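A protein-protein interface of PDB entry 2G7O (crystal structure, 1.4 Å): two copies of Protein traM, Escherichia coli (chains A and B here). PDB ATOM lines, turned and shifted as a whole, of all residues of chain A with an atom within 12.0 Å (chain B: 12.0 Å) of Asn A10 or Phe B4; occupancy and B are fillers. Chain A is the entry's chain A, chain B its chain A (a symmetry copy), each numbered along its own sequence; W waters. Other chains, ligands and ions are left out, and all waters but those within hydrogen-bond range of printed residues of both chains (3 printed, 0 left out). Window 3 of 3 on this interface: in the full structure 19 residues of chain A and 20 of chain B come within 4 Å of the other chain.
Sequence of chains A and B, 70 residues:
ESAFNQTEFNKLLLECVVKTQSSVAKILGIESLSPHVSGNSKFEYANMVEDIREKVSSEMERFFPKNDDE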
ATOM      1  N   ALA A   3       3.273  -4.626  11.553  1.00  0.00           N
ATOM      2  CA  ALA A   3       4.498  -5.493  11.498  1.00  0.00           C
ATOM      3  C   ALA A   3       4.415  -6.589  10.437  1.00  0.00           C
ATOM      4  O   ALA A   3       3.963  -7.706  10.725  1.00  0.00           O
ATOM      5  CB  ALA A   3       4.775  -6.099  12.869  1.00  0.00           C
ATOM      6  N   PHE A   4       4.849  -6.264   9.214  1.00  0.00           N
ATOM      7  CA  PHE A   4       4.759  -7.189   8.085  1.00  0.00           C
ATOM      8  C   PHE A   4       5.794  -8.303   8.171  1.00  0.00           C
ATOM      9  O   PHE A   4       7.003  -8.046   8.164  1.00  0.00           O
ATOM     10  CB  PHE A   4       4.894  -6.454   6.749  1.00  0.00           C
ATOM     11  CG  PHE A   4       4.649  -7.335   5.548  1.00  0.00           C
ATOM     12  CD1 PHE A   4       3.362  -7.737   5.221  1.00  0.00           C
ATOM     13  CD2 PHE A   4       5.708  -7.757   4.748  1.00  0.00           C
ATOM     14  CE1 PHE A   4       3.127  -8.552   4.121  1.00  0.00           C
ATOM     15  CE2 PHE A   4       5.483  -8.572   3.646  1.00  0.00           C
ATOM     16  CZ  PHE A   4       4.184  -8.964   3.332  1.00  0.00           C
ATOM     17  N   ASN A   5       5.297  -9.536   8.234  1.00  0.00           N
ATOM     18  CA  ASN A   5       6.148 -10.703   8.364  1.00  0.00           C
ATOM     19  C   ASN A   5       6.636 -11.170   7.001  1.00  0.00           C
ATOM     20  O   ASN A   5       6.028 -12.034   6.365  1.00  0.00           O
ATOM     21  CB  ASN A   5       5.418 -11.831   9.100  1.00  0.00           C
ATOM     22  CG  ASN A   5       6.361 -12.925   9.575  1.00  0.00           C
ATOM     23  OD1 ASN A   5       7.470 -13.097   9.046  1.00  0.00           O
ATOM     24  ND2 ASN A   5       5.930 -13.668  10.588  1.00  0.00           N
ATOM     25  N   GLN A   6       7.754 -10.591   6.577  1.00  0.00           N
ATOM     26  CA  GLN A   6       8.346 -10.901   5.271  1.00  0.00           C
ATOM     27  C   GLN A   6       8.706 -12.385   5.160  1.00  0.00           C
ATOM     28  O   GLN A   6       8.515 -12.984   4.108  1.00  0.00           O
ATOM     29  CB  GLN A   6       9.565  -9.999   4.990  1.00  0.00           C
ATOM     30  CG  GLN A   6      10.113 -10.130   3.568  1.00  0.00           C
ATOM     31  CD  GLN A   6       9.149  -9.618   2.512  1.00  0.00           C
ATOM     32  OE1 GLN A   6       8.631  -8.504   2.634  1.00  0.00           O
ATOM     33  NE2 GLN A   6       8.902 -10.419   1.474  1.00  0.00           N
ATOM     34  N   THR A   7       9.192 -12.984   6.242  1.00  0.00           N
ATOM     35  CA  THR A   7       9.583 -14.391   6.217  1.00  0.00           C
ATOM     36  C   THR A   7       8.378 -15.298   5.940  1.00  0.00           C
ATOM     37  O   THR A   7       8.422 -16.171   5.067  1.00  0.00           O
ATOM     38  CB  THR A   7      10.288 -14.813   7.515  1.00  0.00           C
ATOM     39  OG1 THR A   7      11.500 -14.069   7.650  1.00  0.00           O
ATOM     40  CG2 THR A   7      10.589 -16.297   7.491  1.00  0.00           C
ATOM     41  N   GLU A   8       7.288 -15.071   6.666  1.00  0.00           N
ATOM     42  CA  GLU A   8       6.076 -15.855   6.447  1.00  0.00           C
ATOM     43  C   GLU A   8       5.470 -15.608   5.060  1.00  0.00           C
ATOM     44  O   GLU A   8       4.950 -16.524   4.432  1.00  0.00           O
ATOM     45  CB  GLU A   8       5.061 -15.619   7.572  1.00  0.00           C
ATOM     46  CG  GLU A   8       5.484 -16.246   8.905  1.00  0.00           C
ATOM     47  CD  GLU A   8       5.524 -17.762   8.878  1.00  0.00           C
ATOM     48  OE1 GLU A   8       4.548 -18.395   8.433  1.00  0.00           O
ATOM     49  OE2 GLU A   8       6.548 -18.327   9.318  1.00  0.00           O
ATOM     50  N   PHE A   9       5.569 -14.367   4.578  1.00  0.00           N
ATOM     51  CA  PHE A   9       5.104 -14.049   3.224  1.00  0.00           C
ATOM     52  C   PHE A   9       5.927 -14.843   2.212  1.00  0.00           C
ATOM     53  O   PHE A   9       5.382 -15.489   1.325  1.00  0.00           O
ATOM     54  CB  PHE A   9       5.183 -12.526   2.982  1.00  0.00           C
ATOM     55  CG  PHE A   9       4.702 -12.085   1.621  1.00  0.00           C
ATOM     56  CD1 PHE A   9       5.581 -12.004   0.546  1.00  0.00           C
ATOM     57  CD2 PHE A   9       3.366 -11.748   1.426  1.00  0.00           C
ATOM     58  CE1 PHE A   9       5.126 -11.598  -0.707  1.00  0.00           C
ATOM     59  CE2 PHE A   9       2.908 -11.316   0.182  1.00  0.00           C
ATOM     60  CZ  PHE A   9       3.785 -11.227  -0.871  1.00  0.00           C
ATOM     61  N   ASN A  10       7.250 -14.818   2.364  1.00  0.00           N
ATOM     62  CA  ASN A  10       8.156 -15.585   1.495  1.00  0.00           C
ATOM     63  C   ASN A  10       7.848 -17.068   1.516  1.00  0.00           C
ATOM     64  O   ASN A  10       7.927 -17.723   0.483  1.00  0.00           O
ATOM     65  CB  ASN A  10       9.630 -15.367   1.895  1.00  0.00           C
ATOM     66  CG  ASN A  10      10.144 -13.985   1.568  1.00  0.00           C
ATOM     67  OD1 ASN A  10       9.542 -13.257   0.776  1.00  0.00           O
ATOM     68  ND2 ASN A  10      11.272 -13.624   2.173  1.00  0.00           N
ATOM     69  N   LYS A  11       7.528 -17.616   2.687  1.00  0.00           N
ATOM     70  CA  LYS A  11       7.193 -19.033   2.811  1.00  0.00           C
ATOM     71  C   LYS A  11       5.946 -19.363   2.020  1.00  0.00           C
ATOM     72  O   LYS A  11       5.903 -20.373   1.317  1.00  0.00           O
ATOM     73  CB  LYS A  11       6.981 -19.435   4.269  1.00  0.00           C
ATOM     74  CG  LYS A  11       8.249 -19.480   5.065  1.00  0.00           C
ATOM     75  CD  LYS A  11       7.986 -19.645   6.550  1.00  0.00           C
ATOM     76  CE  LYS A  11       7.489 -21.030   6.886  1.00  0.00           C
ATOM     77  NZ  LYS A  11       7.429 -21.195   8.367  1.00  0.00           N
ATOM     78  N   LEU A  12       4.910 -18.531   2.146  1.00  0.00           N
ATOM     79  CA  LEU A  12       3.674 -18.760   1.387  1.00  0.00           C
ATOM     80  C   LEU A  12       3.928 -18.628  -0.113  1.00  0.00           C
ATOM     81  O   LEU A  12       3.451 -19.468  -0.924  1.00  0.00           O
ATOM     82  CB  LEU A  12       2.562 -17.820   1.848  1.00  0.00           C
ATOM     83  CG  LEU A  12       1.244 -17.985   1.077  1.00  0.00           C
ATOM     84  CD1 LEU A  12       0.729 -19.436   1.131  1.00  0.00           C
ATOM     85  CD2 LEU A  12       0.220 -17.041   1.676  1.00  0.00           C
ATOM     86  N   LEU A  13       4.658 -17.595  -0.510  1.00  0.00           N
ATOM     87  CA  LEU A  13       4.984 -17.371  -1.917  1.00  0.00           C
ATOM     88  C   LEU A  13       5.701 -18.581  -2.496  1.00  0.00           C
ATOM     89  O   LEU A  13       5.332 -19.090  -3.578  1.00  0.00           O
ATOM     90  CB  LEU A  13       5.852 -16.121  -2.045  1.00  0.00           C
ATOM     91  CG  LEU A  13       6.430 -15.724  -3.386  1.00  0.00           C
ATOM     92  CD1 LEU A  13       5.291 -15.562  -4.400  1.00  0.00           C
ATOM     93  CD2 LEU A  13       7.237 -14.440  -3.255  1.00  0.00           C
ATOM     94  N   LEU A  14       6.709 -19.076  -1.795  1.00  0.00           N
ATOM     95  CA  LEU A  14       7.482 -20.204  -2.302  1.00  0.00           C
ATOM     96  C   LEU A  14       6.634 -21.468  -2.374  1.00  0.00           C
ATOM     97  O   LEU A  14       6.670 -22.187  -3.392  1.00  0.00           O
ATOM     98  CB  LEU A  14       8.721 -20.435  -1.441  1.00  0.00           C
ATOM     99  CG  LEU A  14       9.747 -21.307  -2.176  1.00  0.00           C
ATOM    100  CD1 LEU A  14      10.215 -20.630  -3.499  1.00  0.00           C
ATOM    101  CD2 LEU A  14      10.927 -21.605  -1.261  1.00  0.00           C
ATOM    102  N   GLU A  15       5.867 -21.759  -1.332  1.00  0.00           N
ATOM    103  CA  GLU A  15       5.027 -22.950  -1.352  1.00  0.00           C
ATOM    104  C   GLU A  15       4.091 -22.894  -2.545  1.00  0.00           C
ATOM    105  O   GLU A  15       3.937 -23.874  -3.281  1.00  0.00           O
ATOM    106  CB  GLU A  15       4.210 -23.084  -0.056  1.00  0.00           C
ATOM    107  CG  GLU A  15       3.452 -24.422  -0.002  1.00  0.00           C
ATOM    108  CD  GLU A  15       2.491 -24.567   1.171  1.00  0.00           C
ATOM    109  OE1 GLU A  15       2.655 -23.870   2.193  1.00  0.00           O
ATOM    110  OE2 GLU A  15       1.577 -25.432   1.078  1.00  0.00           O
ATOM    111  N   CYS A  16       3.461 -21.750  -2.760  1.00  0.00           N
ATOM    112  CA  CYS A  16       2.521 -21.620  -3.873  1.00  0.00           C
ATOM    113  C   CYS A  16       3.220 -21.815  -5.219  1.00  0.00           C
ATOM    114  O   CYS A  16       2.752 -22.595  -6.055  1.00  0.00           O
ATOM    115  CB  CYS A  16       1.824 -20.256  -3.851  1.00  0.00           C
ATOM    116  SG  CYS A  16       0.575 -20.100  -2.608  1.00  0.00           S
ATOM    117  N   VAL A  17       4.312 -21.116  -5.481  1.00  0.00           N
ATOM    118  CA  VAL A  17       4.907 -21.182  -6.820  1.00  0.00           C
ATOM    119  C   VAL A  17       5.536 -22.546  -7.091  1.00  0.00           C
ATOM    120  O   VAL A  17       5.470 -23.047  -8.220  1.00  0.00           O
ATOM    121  CB  VAL A  17       5.904 -19.994  -7.149  1.00  0.00           C
ATOM    122  CG1 VAL A  17       5.182 -18.646  -7.021  1.00  0.00           C
ATOM    123  CG2 VAL A  17       7.226 -20.050  -6.374  1.00  0.00           C
ATOM    124  N   VAL A  18       6.149 -23.172  -6.092  1.00  0.00           N
ATOM    125  CA  VAL A  18       6.728 -24.500  -6.283  1.00  0.00           C
ATOM    126  C   VAL A  18       5.614 -25.531  -6.491  1.00  0.00           C
ATOM    127  O   VAL A  18       5.704 -26.395  -7.383  1.00  0.00           O
ATOM    128  CB  VAL A  18       7.651 -24.899  -5.115  1.00  0.00           C
ATOM    129  CG1 VAL A  18       8.111 -26.354  -5.246  1.00  0.00           C
ATOM    130  CG2 VAL A  18       8.850 -23.952  -5.019  1.00  0.00           C
ATOM    131  N   LYS A  19       4.556 -25.453  -5.683  1.00  0.00           N
ATOM    132  CA  LYS A  19       3.447 -26.396  -5.819  1.00  0.00           C
ATOM    133  C   LYS A  19       2.782 -26.220  -7.177  1.00  0.00           C
ATOM    134  O   LYS A  19       2.437 -27.211  -7.846  1.00  0.00           O
ATOM    135  CB  LYS A  19       2.441 -26.213  -4.678  1.00  0.00           C
ATOM    136  CG  LYS A  19       1.504 -27.396  -4.525  1.00  0.00           C
ATOM    137  CD  LYS A  19       0.722 -27.272  -3.214  1.00  0.00           C
ATOM    138  CE  LYS A  19      -0.196 -28.453  -2.988  1.00  0.00           C
ATOM    139  NZ  LYS A  19      -0.879 -28.347  -1.685  1.00  0.00           N
ATOM    140  N   PHE A  64      20.427 -13.716 -13.932  1.00  0.00           N
ATOM    141  CA  PHE A  64      21.451 -14.445 -13.186  1.00  0.00           C
ATOM    142  C   PHE A  64      22.473 -15.037 -14.156  1.00  0.00           C
ATOM    143  O   PHE A  64      22.566 -16.263 -14.278  1.00  0.00           O
ATOM    144  CB  PHE A  64      20.801 -15.537 -12.351  1.00  0.00           C
ATOM    145  CG  PHE A  64      19.691 -15.037 -11.470  1.00  0.00           C
ATOM    146  CD1 PHE A  64      19.982 -14.362 -10.282  1.00  0.00           C
ATOM    147  CD2 PHE A  64      18.363 -15.206 -11.842  1.00  0.00           C
ATOM    148  CE1 PHE A  64      18.943 -13.892  -9.465  1.00  0.00           C
ATOM    149  CE2 PHE A  64      17.329 -14.735 -11.039  1.00  0.00           C
ATOM    150  CZ  PHE A  64      17.626 -14.066  -9.867  1.00  0.00           C
ATOM    151  N   ALA B   3      21.008 -17.091   7.931  1.00  0.00           N
ATOM    152  CA  ALA B   3      21.481 -16.356   6.709  1.00  0.00           C
ATOM    153  C   ALA B   3      20.641 -16.646   5.467  1.00  0.00           C
ATOM    154  O   ALA B   3      20.951 -17.572   4.704  1.00  0.00           O
ATOM    155  CB  ALA B   3      22.949 -16.668   6.444  1.00  0.00           C
ATOM    156  N   PHE B   4      19.579 -15.857   5.271  1.00  0.00           N
ATOM    157  CA  PHE B   4      18.645 -16.068   4.166  1.00  0.00           C
ATOM    158  C   PHE B   4      19.231 -15.635   2.828  1.00  0.00           C
ATOM    159  O   PHE B   4      19.561 -14.460   2.632  1.00  0.00           O
ATOM    160  CB  PHE B   4      17.317 -15.347   4.411  1.00  0.00           C
ATOM    161  CG  PHE B   4      16.260 -15.661   3.379  1.00  0.00           C
ATOM    162  CD1 PHE B   4      15.618 -16.891   3.382  1.00  0.00           C
ATOM    163  CD2 PHE B   4      15.911 -14.723   2.412  1.00  0.00           C
ATOM    164  CE1 PHE B   4      14.648 -17.191   2.435  1.00  0.00           C
ATOM    165  CE2 PHE B   4      14.943 -15.014   1.460  1.00  0.00           C
ATOM    166  CZ  PHE B   4      14.308 -16.253   1.478  1.00  0.00           C
ATOM    167  N   ASN B   5      19.336 -16.598   1.916  1.00  0.00           N
ATOM    168  CA  ASN B   5      19.913 -16.359   0.607  1.00  0.00           C
ATOM    169  C   ASN B   5      18.867 -15.819  -0.355  1.00  0.00           C
ATOM    170  O   ASN B   5      18.223 -16.572  -1.089  1.00  0.00           O
ATOM    171  CB  ASN B   5      20.558 -17.634   0.054  1.00  0.00           C
ATOM    172  CG  ASN B   5      21.476 -17.360  -1.126  1.00  0.00           C
ATOM    173  OD1 ASN B   5      21.355 -16.336  -1.815  1.00  0.00           O
ATOM    174  ND2 ASN B   5      22.411 -18.275  -1.363  1.00  0.00           N
ATOM    175  N   GLN B   6      18.725 -14.497  -0.345  1.00  0.00           N
ATOM    176  CA  GLN B   6      17.739 -13.814  -1.188  1.00  0.00           C
ATOM    177  C   GLN B   6      17.989 -14.085  -2.673  1.00  0.00           C
ATOM    178  O   GLN B   6      17.043 -14.268  -3.431  1.00  0.00           O
ATOM    179  CB  GLN B   6      17.709 -12.301  -0.885  1.00  0.00           C
ATOM    180  CG  GLN B   6      16.571 -11.555  -1.583  1.00  0.00           C
ATOM    181  CD  GLN B   6      15.198 -11.959  -1.075  1.00  0.00           C
ATOM    182  OE1 GLN B   6      14.970 -11.981   0.138  1.00  0.00           O
ATOM    183  NE2 GLN B   6      14.281 -12.277  -1.990  1.00  0.00           N
ATOM    184  N   THR B   7      19.252 -14.145  -3.085  1.00  0.00           N
ATOM    185  CA  THR B   7      19.580 -14.376  -4.489  1.00  0.00           C
ATOM    186  C   THR B   7      19.092 -15.754  -4.953  1.00  0.00           C
ATOM    187  O   THR B   7      18.431 -15.882  -5.990  1.00  0.00           O
ATOM    188  CB  THR B   7      21.083 -14.218  -4.759  1.00  0.00           C
ATOM    189  OG1 THR B   7      21.468 -12.871  -4.481  1.00  0.00           O
ATOM    190  CG2 THR B   7      21.397 -14.561  -6.200  1.00  0.00           C
ATOM    191  N   GLU B   8      19.394 -16.784  -4.169  1.00  0.00           N
ATOM    192  CA  GLU B   8      18.938 -18.130  -4.505  1.00  0.00           C
ATOM    193  C   GLU B   8      17.410 -18.254  -4.451  1.00  0.00           C
ATOM    194  O   GLU B   8      16.809 -18.951  -5.260  1.00  0.00           O
ATOM    195  CB  GLU B   8      19.635 -19.178  -3.630  1.00  0.00           C
ATOM    196  CG  GLU B   8      21.116 -19.361  -3.975  1.00  0.00           C
ATOM    197  CD  GLU B   8      21.352 -19.948  -5.354  1.00  0.00           C
ATOM    198  OE1 GLU B   8      20.733 -20.972  -5.700  1.00  0.00           O
ATOM    199  OE2 GLU B   8      22.175 -19.376  -6.100  1.00  0.00           O
ATOM    200  N   PHE B   9      16.787 -17.545  -3.506  1.00  0.00           N
ATOM    201  CA  PHE B   9      15.323 -17.522  -3.428  1.00  0.00           C
ATOM    202  C   PHE B   9      14.764 -16.899  -4.705  1.00  0.00           C
ATOM    203  O   PHE B   9      13.868 -17.450  -5.334  1.00  0.00           O
ATOM    204  CB  PHE B   9      14.873 -16.768  -2.158  1.00  0.00           C
ATOM    205  CG  PHE B   9      13.377 -16.707  -1.966  1.00  0.00           C
ATOM    206  CD1 PHE B   9      12.633 -15.659  -2.497  1.00  0.00           C
ATOM    207  CD2 PHE B   9      12.722 -17.703  -1.248  1.00  0.00           C
ATOM    208  CE1 PHE B   9      11.252 -15.613  -2.316  1.00  0.00           C
ATOM    209  CE2 PHE B   9      11.344 -17.652  -1.041  1.00  0.00           C
ATOM    210  CZ  PHE B   9      10.619 -16.607  -1.557  1.00  0.00           C
ATOM    211  N   ASN B  10      15.315 -15.755  -5.106  1.00  0.00           N
ATOM    212  CA  ASN B  10      14.910 -15.080  -6.348  1.00  0.00           C
ATOM    213  C   ASN B  10      15.075 -15.970  -7.563  1.00  0.00           C
ATOM    214  O   ASN B  10      14.240 -15.941  -8.458  1.00  0.00           O
ATOM    215  CB  ASN B  10      15.709 -13.778  -6.561  1.00  0.00           C
ATOM    216  CG  ASN B  10      15.339 -12.679  -5.593  1.00  0.00           C
ATOM    217  OD1 ASN B  10      14.290 -12.732  -4.946  1.00  0.00           O
ATOM    218  ND2 ASN B  10      16.199 -11.669  -5.501  1.00  0.00           N
ATOM    219  N   LYS B  11      16.161 -16.740  -7.620  1.00  0.00           N
ATOM    220  CA  LYS B  11      16.403 -17.650  -8.738  1.00  0.00           C
ATOM    221  C   LYS B  11      15.327 -18.711  -8.811  1.00  0.00           C
ATOM    222  O   LYS B  11      14.820 -19.011  -9.893  1.00  0.00           O
ATOM    223  CB  LYS B  11      17.767 -18.328  -8.625  1.00  0.00           C
ATOM    224  CG  LYS B  11      18.915 -17.405  -8.892  1.00  0.00           C
ATOM    225  CD  LYS B  11      20.250 -18.036  -8.542  1.00  0.00           C
ATOM    226  CE  LYS B  11      20.635 -19.123  -9.516  1.00  0.00           C
ATOM    227  NZ  LYS B  11      22.029 -19.574  -9.237  1.00  0.00           N
ATOM    228  N   LEU B  12      14.985 -19.310  -7.668  1.00  0.00           N
ATOM    229  CA  LEU B  12      13.926 -20.326  -7.647  1.00  0.00           C
ATOM    230  C   LEU B  12      12.580 -19.713  -8.028  1.00  0.00           C
ATOM    231  O   LEU B  12      11.809 -20.302  -8.834  1.00  0.00           O
ATOM    232  CB  LEU B  12      13.857 -21.021  -6.289  1.00  0.00           C
ATOM    233  CG  LEU B  12      12.750 -22.081  -6.184  1.00  0.00           C
ATOM    234  CD1 LEU B  12      12.876 -23.148  -7.288  1.00  0.00           C
ATOM    235  CD2 LEU B  12      12.837 -22.727  -4.815  1.00  0.00           C
ATOM    236  N   LEU B  13      12.268 -18.553  -7.468  1.00  0.00           N
ATOM    237  CA  LEU B  13      11.017 -17.859  -7.766  1.00  0.00           C
ATOM    238  C   LEU B  13      10.896 -17.599  -9.260  1.00  0.00           C
ATOM    239  O   LEU B  13       9.852 -17.894  -9.882  1.00  0.00           O
ATOM    240  CB  LEU B  13      10.965 -16.547  -6.986  1.00  0.00           C
ATOM    241  CG  LEU B  13       9.825 -15.574  -7.201  1.00  0.00           C
ATOM    242  CD1 LEU B  13       8.494 -16.286  -6.933  1.00  0.00           C
ATOM    243  CD2 LEU B  13       9.991 -14.359  -6.299  1.00  0.00           C
ATOM    244  N   LEU B  14      11.948 -17.070  -9.866  1.00  0.00           N
ATOM    245  CA  LEU B  14      11.899 -16.742 -11.286  1.00  0.00           C
ATOM    246  C   LEU B  14      11.773 -17.998 -12.140  1.00  0.00           C
ATOM    247  O   LEU B  14      10.949 -18.037 -13.075  1.00  0.00           O
ATOM    248  CB  LEU B  14      13.130 -15.936 -11.692  1.00  0.00           C
ATOM    249  CG  LEU B  14      12.905 -15.228 -13.035  1.00  0.00           C
ATOM    250  CD1 LEU B  14      11.703 -14.240 -12.954  1.00  0.00           C
ATOM    251  CD2 LEU B  14      14.179 -14.514 -13.465  1.00  0.00           C
ATOM    252  N   CYS B  16      10.466 -20.830 -11.383  1.00  0.00           N
ATOM    253  CA  CYS B  16       9.110 -21.357 -11.241  1.00  0.00           C
ATOM    254  C   CYS B  16       8.101 -20.521 -12.029  1.00  0.00           C
ATOM    255  O   CYS B  16       7.299 -21.072 -12.791  1.00  0.00           O
ATOM    256  CB  CYS B  16       8.690 -21.412  -9.768  1.00  0.00           C
ATOM    257  SG  CYS B  16       9.437 -22.727  -8.851  1.00  0.00           S
ATOM    258  N   VAL B  17       8.083 -19.210 -11.859  1.00  0.00           N
ATOM    259  CA  VAL B  17       7.026 -18.414 -12.492  1.00  0.00           C
ATOM    260  C   VAL B  17       7.191 -18.364 -14.008  1.00  0.00           C
ATOM    261  O   VAL B  17       6.197 -18.378 -14.743  1.00  0.00           O
ATOM    262  CB  VAL B  17       6.836 -16.969 -11.868  1.00  0.00           C
ATOM    263  CG1 VAL B  17       6.511 -17.076 -10.373  1.00  0.00           C
ATOM    264  CG2 VAL B  17       7.983 -15.998 -12.171  1.00  0.00           C
HETATM  265  O   HOH W   1      11.418 -12.200  -1.222  1.00  0.00           O
HETATM  266  O   HOH W   2       4.900 -21.395 -10.389  1.00  0.00           O
HETATM  267  O   HOH W   3      12.641 -11.157   1.327  1.00  0.00           O
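SG of Cys B16 lies within hydrogen-bond range of O of Leu B12 (3.4 Å).
The side-chain amide oxygen of Asn A10 sits at hydrogen-bond distance from the side-chain amide nitrogen of Gln A6 (3.0 Å).
OE2 of Glu B8 lies within salt-bridge range of NZ of Lys B11 (3.1 Å).
The side-chain amide nitrogen of Gln B6 lies within hydrogen-bond range of the side-chain amide oxygen of Asn B10.
ND2 of Asn A10 touches CE2 of Phe B4, 3.99 Å away.
Asn A10 touches Phe B9 (O to CZ, 3.6 Å).
CB of Leu A14 touches CE2 of Phe B9, 3.8 Å away.
Leu B12 touches Leu A14.
Val A17 touches Cys B16 (O to CB, 3.9 Å).
Val B17 touches Val A17.
CZ of Phe A64 touches CB of Asn B10, 3.8 Å away.
CD1 of Phe A64 touches CG of Lys B11 (3.5 Å).
CE2 of Phe A64 touches CD2 of Leu B14 (3.98 Å).
Of the printed residues of chain A, Phe B4 touches Asn A10 (3.99 Å).
No residue of chain B comes within 4 Å of Gln A6.
No residue of chain B comes within 4 Å of Thr A7.
No residue of chain B comes within 4 Å of Phe A9.
No residue of chain B comes within 4 Å of Leu A12.
No residue of chain B comes within 4 Å of Leu A13.
Leu A14 touches just these residues of chain B: Phe B9 and Leu B12.
No residue of chain A comes within 4 Å of Asn B5.
Phe B9 touches two residues of chain A.
Of the printed residues of chain A, Cys B16 touches Val A17 (3.9 Å).
Of the printed residues of chain B, Phe A64 touches Asn B10, Lys B11 and Leu B14.
Phe A4 touches none of the printed residues of chain B.
Leu B13 touches none of the printed residues of chain A.
Printed residues of chain A that touch a printed residue of chain B: Asn A10, Leu A14, Val A17 and Phe A64.
Of the 14 printed residues of chain B, 8 touch a printed residue of chain A.
Hydrophobic or aromatic side chains of chain B within 4 Å of the printed part of chain A: Phe B4, Phe B9, Leu B12, Leu B14 and Val B17.
Asn A10 touches Phe B4, but with the chains exchanged Phe A4 does not touch Asn B10 (13.0 Å).
Leu A14 touches Leu B12, but with the chains exchanged Leu A12 does not touch Leu B14 (12.6 Å).
Val A17 touches Cys B16, but with the chains exchanged Cys A16 does not touch Val B17 (7.7 Å).
Val B17 touches its own counterpart, Val A17.
Positions printed for both chains: 3, 4, 5, 6, 7, 8, 9, 10, 11, 12, 13, 14, 16 and 17.
Of the 9 pairs that touch across the chains among the printed residues, 1 has its exchanged pair printed and touching as well.
Water W3 lies within hydrogen-bond range of the side-chain amide oxygen of Gln B6 (2.7 Å) and the side-chain amide nitrogen of Asn A10 (2.9 Å).
Water W2 lies within hydrogen-bond range of the backbone carbonyl oxygen of Val A17 (2.8 Å) and the backbone carbonyl oxygen of Cys B16 (3.4 Å).
Water W1 lies within hydrogen-bond range of OD1 of Asn A10 (2.9 Å) and NE2 of Gln B6 (3.0 Å).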
